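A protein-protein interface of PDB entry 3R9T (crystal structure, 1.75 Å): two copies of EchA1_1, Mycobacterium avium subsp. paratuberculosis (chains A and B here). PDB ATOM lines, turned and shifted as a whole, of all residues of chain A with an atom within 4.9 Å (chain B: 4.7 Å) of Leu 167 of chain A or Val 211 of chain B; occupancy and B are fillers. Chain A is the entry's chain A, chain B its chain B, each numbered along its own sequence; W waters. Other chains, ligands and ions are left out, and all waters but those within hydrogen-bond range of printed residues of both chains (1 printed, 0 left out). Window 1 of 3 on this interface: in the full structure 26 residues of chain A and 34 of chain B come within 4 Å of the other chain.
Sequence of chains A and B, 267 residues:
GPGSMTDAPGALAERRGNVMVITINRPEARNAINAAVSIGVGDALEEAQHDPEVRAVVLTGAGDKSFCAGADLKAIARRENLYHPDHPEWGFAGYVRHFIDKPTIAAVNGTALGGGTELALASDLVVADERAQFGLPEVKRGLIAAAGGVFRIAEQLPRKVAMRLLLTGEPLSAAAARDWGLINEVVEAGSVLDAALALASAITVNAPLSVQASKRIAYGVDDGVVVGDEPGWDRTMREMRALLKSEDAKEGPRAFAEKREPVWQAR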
ATOM      1  N   VAL A 139      21.537   5.673 -11.651  1.00  0.00           N
ATOM      2  CA  VAL A 139      22.552   4.619 -11.527  1.00  0.00           C
ATOM      3  C   VAL A 139      23.499   4.501 -12.723  1.00  0.00           C
ATOM      4  O   VAL A 139      24.605   3.988 -12.591  1.00  0.00           O
ATOM      5  CB  VAL A 139      21.918   3.258 -11.208  1.00  0.00           C
ATOM      6  CG1 VAL A 139      21.340   3.298  -9.793  1.00  0.00           C
ATOM      7  CG2 VAL A 139      20.899   2.829 -12.294  1.00  0.00           C
ATOM      8  N   MET A 163      12.369  -2.712  -7.990  1.00  0.00           N
ATOM      9  CA  MET A 163      13.787  -2.998  -7.863  1.00  0.00           C
ATOM     10  C   MET A 163      14.417  -3.111  -9.253  1.00  0.00           C
ATOM     11  O   MET A 163      15.546  -2.676  -9.454  1.00  0.00           O
ATOM     12  CB  MET A 163      14.049  -4.252  -7.032  1.00  0.00           C
ATOM     13  CG  MET A 163      13.643  -4.120  -5.581  1.00  0.00           C
ATOM     14  SD  MET A 163      14.406  -2.728  -4.729  1.00  0.00           S
ATOM     15  CE  MET A 163      16.060  -3.082  -5.223  1.00  0.00           C
ATOM     16  N   ARG A 164      13.691  -3.644 -10.228  1.00  0.00           N
ATOM     17  CA  ARG A 164      14.205  -3.692 -11.608  1.00  0.00           C
ATOM     18  C   ARG A 164      14.446  -2.273 -12.130  1.00  0.00           C
ATOM     19  O   ARG A 164      15.483  -1.996 -12.744  1.00  0.00           O
ATOM     20  CB  ARG A 164      13.266  -4.478 -12.548  1.00  0.00           C
ATOM     21  CG  ARG A 164      13.743  -4.575 -14.040  1.00  0.00           C
ATOM     22  CD  ARG A 164      12.763  -5.343 -15.000  1.00  0.00           C
ATOM     23  NE  ARG A 164      13.302  -6.653 -15.384  1.00  0.00           N
ATOM     24  CZ  ARG A 164      12.697  -7.610 -16.104  1.00  0.00           C
ATOM     25  NH1 ARG A 164      13.356  -8.729 -16.310  1.00  0.00           N
ATOM     26  NH2 ARG A 164      11.474  -7.499 -16.609  1.00  0.00           N
ATOM     27  N   LEU A 165      13.492  -1.383 -11.895  1.00  0.00           N
ATOM     28  CA  LEU A 165      13.621   0.003 -12.339  1.00  0.00           C
ATOM     29  C   LEU A 165      14.819   0.678 -11.693  1.00  0.00           C
ATOM     30  O   LEU A 165      15.642   1.333 -12.348  1.00  0.00           O
ATOM     31  CB  LEU A 165      12.322   0.751 -12.028  1.00  0.00           C
ATOM     32  CG  LEU A 165      12.114   2.128 -12.638  1.00  0.00           C
ATOM     33  CD1 LEU A 165      10.622   2.375 -12.864  1.00  0.00           C
ATOM     34  CD2 LEU A 165      12.684   3.195 -11.731  1.00  0.00           C
ATOM     35  N   LEU A 166      14.928   0.487 -10.387  1.00  0.00           N
ATOM     36  CA  LEU A 166      15.958   1.128  -9.610  1.00  0.00           C
ATOM     37  C   LEU A 166      17.358   0.658  -9.981  1.00  0.00           C
ATOM     38  O   LEU A 166      18.251   1.494 -10.134  1.00  0.00           O
ATOM     39  CB  LEU A 166      15.652   0.913  -8.125  1.00  0.00           C
ATOM     40  CG  LEU A 166      16.558   1.609  -7.121  1.00  0.00           C
ATOM     41  CD1 LEU A 166      16.375   3.131  -7.255  1.00  0.00           C
ATOM     42  CD2 LEU A 166      16.225   1.127  -5.736  1.00  0.00           C
ATOM     43  N   LEU A 167      17.557  -0.647 -10.140  1.00  0.00           N
ATOM     44  CA  LEU A 167      18.883  -1.196 -10.313  1.00  0.00           C
ATOM     45  C   LEU A 167      19.335  -1.212 -11.771  1.00  0.00           C
ATOM     46  O   LEU A 167      20.527  -1.076 -12.022  1.00  0.00           O
ATOM     47  CB  LEU A 167      18.966  -2.586  -9.701  1.00  0.00           C
ATOM     48  CG  LEU A 167      18.584  -2.664  -8.218  1.00  0.00           C
ATOM     49  CD1 LEU A 167      18.650  -4.103  -7.736  1.00  0.00           C
ATOM     50  CD2 LEU A 167      19.451  -1.754  -7.309  1.00  0.00           C
ATOM     51  N   THR A 168      18.409  -1.337 -12.730  1.00  0.00           N
ATOM     52  CA  THR A 168      18.799  -1.301 -14.162  1.00  0.00           C
ATOM     53  C   THR A 168      18.936   0.134 -14.696  1.00  0.00           C
ATOM     54  O   THR A 168      19.708   0.385 -15.618  1.00  0.00           O
ATOM     55  CB  THR A 168      17.789  -2.054 -15.098  1.00  0.00           C
ATOM     56  OG1 THR A 168      16.518  -1.386 -15.112  1.00  0.00           O
ATOM     57  CG2 THR A 168      17.625  -3.551 -14.686  1.00  0.00           C
ATOM     58  N   GLY A 169      18.176   1.066 -14.125  1.00  0.00           N
ATOM     59  CA  GLY A 169      18.084   2.423 -14.641  1.00  0.00           C
ATOM     60  C   GLY A 169      17.324   2.522 -15.963  1.00  0.00           C
ATOM     61  O   GLY A 169      17.376   3.563 -16.638  1.00  0.00           O
ATOM     62  N   ARG B  55      29.883  -8.302  -9.502  1.00  0.00           N
ATOM     63  CA  ARG B  55      28.926  -7.195  -9.641  1.00  0.00           C
ATOM     64  C   ARG B  55      27.462  -7.597  -9.450  1.00  0.00           C
ATOM     65  O   ARG B  55      26.590  -6.729  -9.307  1.00  0.00           O
ATOM     66  CB  ARG B  55      29.060  -6.548 -11.023  1.00  0.00           C
ATOM     67  CG  ARG B  55      30.388  -5.840 -11.274  1.00  0.00           C
ATOM     68  CD  ARG B  55      30.618  -4.660 -10.338  1.00  0.00           C
ATOM     69  NE  ARG B  55      29.406  -3.847 -10.300  1.00  0.00           N
ATOM     70  CZ  ARG B  55      29.045  -2.925 -11.193  1.00  0.00           C
ATOM     71  NH1 ARG B  55      29.839  -2.578 -12.201  1.00  0.00           N
ATOM     72  NH2 ARG B  55      27.873  -2.312 -11.041  1.00  0.00           N
ATOM     73  N   ASP B 101      25.206  -6.065  -0.594  1.00  0.00           N
ATOM     74  CA  ASP B 101      25.188  -4.819  -1.371  1.00  0.00           C
ATOM     75  C   ASP B 101      24.967  -5.001  -2.862  1.00  0.00           C
ATOM     76  O   ASP B 101      24.650  -4.044  -3.604  1.00  0.00           O
ATOM     77  CB  ASP B 101      26.567  -4.154  -1.245  1.00  0.00           C
ATOM     78  CG  ASP B 101      26.815  -3.554   0.114  1.00  0.00           C
ATOM     79  OD1 ASP B 101      25.842  -3.156   0.786  1.00  0.00           O
ATOM     80  OD2 ASP B 101      27.998  -3.464   0.504  1.00  0.00           O
ATOM     81  N   PRO B 103      23.397  -6.842  -6.345  1.00  0.00           N
ATOM     82  CA  PRO B 103      22.122  -7.390  -6.759  1.00  0.00           C
ATOM     83  C   PRO B 103      22.090  -8.914  -6.806  1.00  0.00           C
ATOM     84  O   PRO B 103      23.067  -9.556  -7.240  1.00  0.00           O
ATOM     85  CB  PRO B 103      21.922  -6.801  -8.167  1.00  0.00           C
ATOM     86  CG  PRO B 103      23.317  -6.478  -8.643  1.00  0.00           C
ATOM     87  CD  PRO B 103      24.010  -6.020  -7.406  1.00  0.00           C
ATOM     88  N   ASP B 124      16.493  -9.860  -4.942  1.00  0.00           N
ATOM     89  CA  ASP B 124      16.076  -8.579  -5.477  1.00  0.00           C
ATOM     90  C   ASP B 124      15.124  -8.714  -6.667  1.00  0.00           C
ATOM     91  O   ASP B 124      14.155  -7.952  -6.779  1.00  0.00           O
ATOM     92  CB  ASP B 124      17.270  -7.732  -5.894  1.00  0.00           C
ATOM     93  CG  ASP B 124      18.182  -7.407  -4.753  1.00  0.00           C
ATOM     94  OD1 ASP B 124      17.658  -7.066  -3.663  1.00  0.00           O
ATOM     95  OD2 ASP B 124      19.423  -7.471  -4.970  1.00  0.00           O
ATOM     96  N   ALA B 202      22.083  -5.998 -17.411  1.00  0.00           N
ATOM     97  CA  ALA B 202      21.377  -4.707 -17.402  1.00  0.00           C
ATOM     98  C   ALA B 202      21.648  -3.876 -16.150  1.00  0.00           C
ATOM     99  O   ALA B 202      21.369  -2.678 -16.143  1.00  0.00           O
ATOM    100  CB  ALA B 202      19.844  -4.915 -17.577  1.00  0.00           C
ATOM    101  N   ILE B 203      22.165  -4.522 -15.103  1.00  0.00           N
ATOM    102  CA  ILE B 203      22.523  -3.880 -13.838  1.00  0.00           C
ATOM    103  C   ILE B 203      24.020  -3.645 -13.741  1.00  0.00           C
ATOM    104  O   ILE B 203      24.433  -2.570 -13.319  1.00  0.00           O
ATOM    105  CB  ILE B 203      22.065  -4.738 -12.636  1.00  0.00           C
ATOM    106  CG1 ILE B 203      20.557  -4.985 -12.713  1.00  0.00           C
ATOM    107  CG2 ILE B 203      22.453  -4.064 -11.277  1.00  0.00           C
ATOM    108  CD1 ILE B 203      20.089  -6.072 -11.737  1.00  0.00           C
ATOM    109  N   ASN B 206      25.945  -0.604 -14.859  1.00  0.00           N
ATOM    110  CA  ASN B 206      25.726   0.627 -14.093  1.00  0.00           C
ATOM    111  C   ASN B 206      26.799   0.834 -13.035  1.00  0.00           C
ATOM    112  O   ASN B 206      27.585  -0.076 -12.749  1.00  0.00           O
ATOM    113  CB  ASN B 206      24.325   0.629 -13.483  1.00  0.00           C
ATOM    114  CG  ASN B 206      23.239   0.544 -14.549  1.00  0.00           C
ATOM    115  OD1 ASN B 206      23.407   1.064 -15.673  1.00  0.00           O
ATOM    116  ND2 ASN B 206      22.125  -0.112 -14.218  1.00  0.00           N
ATOM    117  N   ALA B 207      26.840   2.042 -12.479  1.00  0.00           N
ATOM    118  CA  ALA B 207      27.866   2.417 -11.512  1.00  0.00           C
ATOM    119  C   ALA B 207      27.709   1.603 -10.239  1.00  0.00           C
ATOM    120  O   ALA B 207      26.640   1.621  -9.647  1.00  0.00           O
ATOM    121  CB  ALA B 207      27.793   3.897 -11.213  1.00  0.00           C
ATOM    122  N   PRO B 208      28.759   0.852  -9.843  1.00  0.00           N
ATOM    123  CA  PRO B 208      28.639  -0.060  -8.693  1.00  0.00           C
ATOM    124  C   PRO B 208      28.249   0.622  -7.394  1.00  0.00           C
ATOM    125  O   PRO B 208      27.417   0.116  -6.657  1.00  0.00           O
ATOM    126  CB  PRO B 208      30.051  -0.657  -8.550  1.00  0.00           C
ATOM    127  CG  PRO B 208      30.939   0.232  -9.331  1.00  0.00           C
ATOM    128  CD  PRO B 208      30.094   0.750 -10.465  1.00  0.00           C
ATOM    129  N   LEU B 209      28.874   1.746  -7.087  1.00  0.00           N
ATOM    130  CA  LEU B 209      28.548   2.416  -5.832  1.00  0.00           C
ATOM    131  C   LEU B 209      27.106   2.927  -5.797  1.00  0.00           C
ATOM    132  O   LEU B 209      26.488   2.975  -4.733  1.00  0.00           O
ATOM    133  CB  LEU B 209      29.497   3.578  -5.557  1.00  0.00           C
ATOM    134  CG  LEU B 209      30.982   3.222  -5.400  1.00  0.00           C
ATOM    135  CD1 LEU B 209      31.815   4.508  -5.315  1.00  0.00           C
ATOM    136  CD2 LEU B 209      31.192   2.324  -4.188  1.00  0.00           C
ATOM    137  N   SER B 210      26.582   3.305  -6.957  1.00  0.00           N
ATOM    138  CA  SER B 210      25.193   3.755  -7.075  1.00  0.00           C
ATOM    139  C   SER B 210      24.230   2.598  -6.865  1.00  0.00           C
ATOM    140  O   SER B 210      23.212   2.743  -6.203  1.00  0.00           O
ATOM    141  CB  SER B 210      24.936   4.332  -8.463  1.00  0.00           C
ATOM    142  OG  SER B 210      25.722   5.474  -8.699  1.00  0.00           O
ATOM    143  N   VAL B 211      24.538   1.444  -7.446  1.00  0.00           N
ATOM    144  CA  VAL B 211      23.658   0.256  -7.319  1.00  0.00           C
ATOM    145  C   VAL B 211      23.610  -0.206  -5.849  1.00  0.00           C
ATOM    146  O   VAL B 211      22.534  -0.487  -5.286  1.00  0.00           O
ATOM    147  CB  VAL B 211      24.138  -0.888  -8.273  1.00  0.00           C
ATOM    148  CG1 VAL B 211      23.462  -2.257  -7.947  1.00  0.00           C
ATOM    149  CG2 VAL B 211      23.931  -0.494  -9.741  1.00  0.00           C
ATOM    150  N   GLN B 212      24.795  -0.249  -5.245  1.00  0.00           N
ATOM    151  CA  GLN B 212      24.990  -0.665  -3.848  1.00  0.00           C
ATOM    152  C   GLN B 212      24.267   0.277  -2.900  1.00  0.00           C
ATOM    153  O   GLN B 212      23.512  -0.169  -2.024  1.00  0.00           O
ATOM    154  CB  GLN B 212      26.486  -0.767  -3.533  1.00  0.00           C
ATOM    155  CG  GLN B 212      27.079  -1.934  -4.278  1.00  0.00           C
ATOM    156  CD  GLN B 212      28.584  -2.020  -4.307  1.00  0.00           C
ATOM    157  OE1 GLN B 212      29.131  -2.788  -5.104  1.00  0.00           O
ATOM    158  NE2 GLN B 212      29.264  -1.270  -3.462  1.00  0.00           N
ATOM    159  N   ALA B 213      24.450   1.577  -3.108  1.00  0.00           N
ATOM    160  CA  ALA B 213      23.787   2.572  -2.274  1.00  0.00           C
ATOM    161  C   ALA B 213      22.269   2.510  -2.446  1.00  0.00           C
ATOM    162  O   ALA B 213      21.508   2.643  -1.478  1.00  0.00           O
ATOM    163  CB  ALA B 213      24.284   3.965  -2.592  1.00  0.00           C
ATOM    164  N   SER B 214      21.817   2.321  -3.688  1.00  0.00           N
ATOM    165  CA  SER B 214      20.381   2.232  -3.969  1.00  0.00           C
ATOM    166  C   SER B 214      19.758   1.047  -3.252  1.00  0.00           C
ATOM    167  O   SER B 214      18.677   1.161  -2.682  1.00  0.00           O
ATOM    168  CB  SER B 214      20.099   2.121  -5.477  1.00  0.00           C
ATOM    169  OG  SER B 214      20.488   3.292  -6.151  1.00  0.00           O
ATOM    170  N   LYS B 215      20.454  -0.084  -3.251  1.00  0.00           N
ATOM    171  CA  LYS B 215      19.981  -1.251  -2.493  1.00  0.00           C
ATOM    172  C   LYS B 215      19.879  -0.990  -1.008  1.00  0.00           C
ATOM    173  O   LYS B 215      18.875  -1.331  -0.394  1.00  0.00           O
ATOM    174  CB  LYS B 215      20.899  -2.470  -2.680  1.00  0.00           C
ATOM    175  CG  LYS B 215      20.489  -3.432  -3.743  1.00  0.00           C
ATOM    176  CD  LYS B 215      21.182  -4.828  -3.596  1.00  0.00           C
ATOM    177  CE  LYS B 215      20.586  -5.729  -2.521  1.00  0.00           C
ATOM    178  NZ  LYS B 215      20.979  -7.196  -2.721  1.00  0.00           N
HETATM  179  O   HOH W   1      20.780  -1.354 -18.348  1.00  0.00           O
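The side-chain amide nitrogen (ND2) of Asn 206 of chain B is in hydrogen-bond range of the backbone carbonyl oxygen (O) of Thr 168 of chain A, 2.8 Å away. The backbone carbonyl oxygen of Leu 167 of chain A lies within hydrogen-bond range of the side-chain amide nitrogen of Asn 206 of chain B (2.9 Å). The backbone NH (N) of Ala 207 of chain B lies within hydrogen-bond range of the backbone carbonyl oxygen (O) of Val 139 of chain A (3.0 Å).
NH2 of Arg 55 of chain B lies within hydrogen-bond range of O of Asn 206 of chain B (2.8 Å). NZ of Lys 215 of chain B is in salt-bridge range of OD2 of Asp 124 of chain B, 2.7 Å away. The backbone carbonyl oxygen (O) of Ser 210 of chain B sits at hydrogen-bond distance from the side-chain hydroxyl (OG) of Ser 214 of chain B (2.8 Å). The side-chain amide nitrogen (ND2) of Asn 206 of chain B sits close to the backbone carbonyl oxygen (O) of Ile 203 of chain B (3.5 Å). ND2 of Asn 206 of chain B sits at hydrogen-bond distance from O of Ala 202 of chain B. The side-chain hydroxyl (OG1) of Thr 168 of chain A is in hydrogen-bond range of the backbone carbonyl oxygen (O) of Arg 164 of chain A.
Among the printed residues, pairs that only touch across the chains: Val 139 of chain A with Asn 206 of chain B, Thr 168 of chain A with Ala 202 of chain B, Leu 167 of chain A with Ile 203 of chain B, Met 163 of chain A with Asp 124 of chain B, Val 139 of chain A with Ser 214 of chain B, Thr 168 of chain A with Ile 203 of chain B, Val 139 of chain A with Ser 210 of chain B, Leu 167 of chain A with Val 211 of chain B and Leu 166 of chain A with Ser 214 of chain B.
Of chain B, only Ile 203, Asn 206 and Val 211 come within 4 Å of Leu 167 of chain A. Val 211 of chain B touches just one residue of chain A: Leu 167. Of the printed residues of chain A, Ala 207 of chain B touches Val 139. Of the printed residues of chain B, Met 163 of chain A touches Asp 124. Of the printed residues of chain A, Asp 124 of chain B touches Met 163 (3.7 Å). Of the printed residues of chain A, Asn 206 of chain B touches Val 139 (3.5 Å), Leu 167 (2.9 Å) and Thr 168 (2.8 Å). Printed residues of chain A within 4 Å of Ala 202 of chain B: Thr 168 (3.5 Å). Arg 55 of chain B touches none of the printed residues of chain A. Ala 213 of chain B touches none of the printed residues of chain A. The nearest residue of chain A that does not touch Val 211 of chain B is Val 139 of chain A (4.4 Å). The nearest printed residue of chain B that does not touch Met 163 of chain A is Lys 215 of chain B (4.7 Å).
Of the 8 printed residues of chain A, 5 touch a printed residue of chain B. Printed residues of chain B that touch a printed residue of chain A: Asp 124, Ala 202, Ile 203, Asn 206, Ala 207, Ser 210, Val 211 and Ser 214. Hydrophobic or aromatic side chains of chain B that line the printed part of chain A: Ala 202, Ile 203 and Ala 207. Along chain B the printed residues that touch a printed residue of chain A span positions 124 to 214. Among the printed residues, no Asp or Glu carboxylate lies within 4 Å of a Lys or Arg side-chain nitrogen of the other chain.
No position is printed for both chains. Of the 12 pairs that touch across the chains among the printed residues, none has its exchanged pair printed and touching as well.
Water W1 lies within hydrogen-bond range of O of Ala 202 of chain B (2.6 Å) and O of Thr 168 of chain A (3.4 Å).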
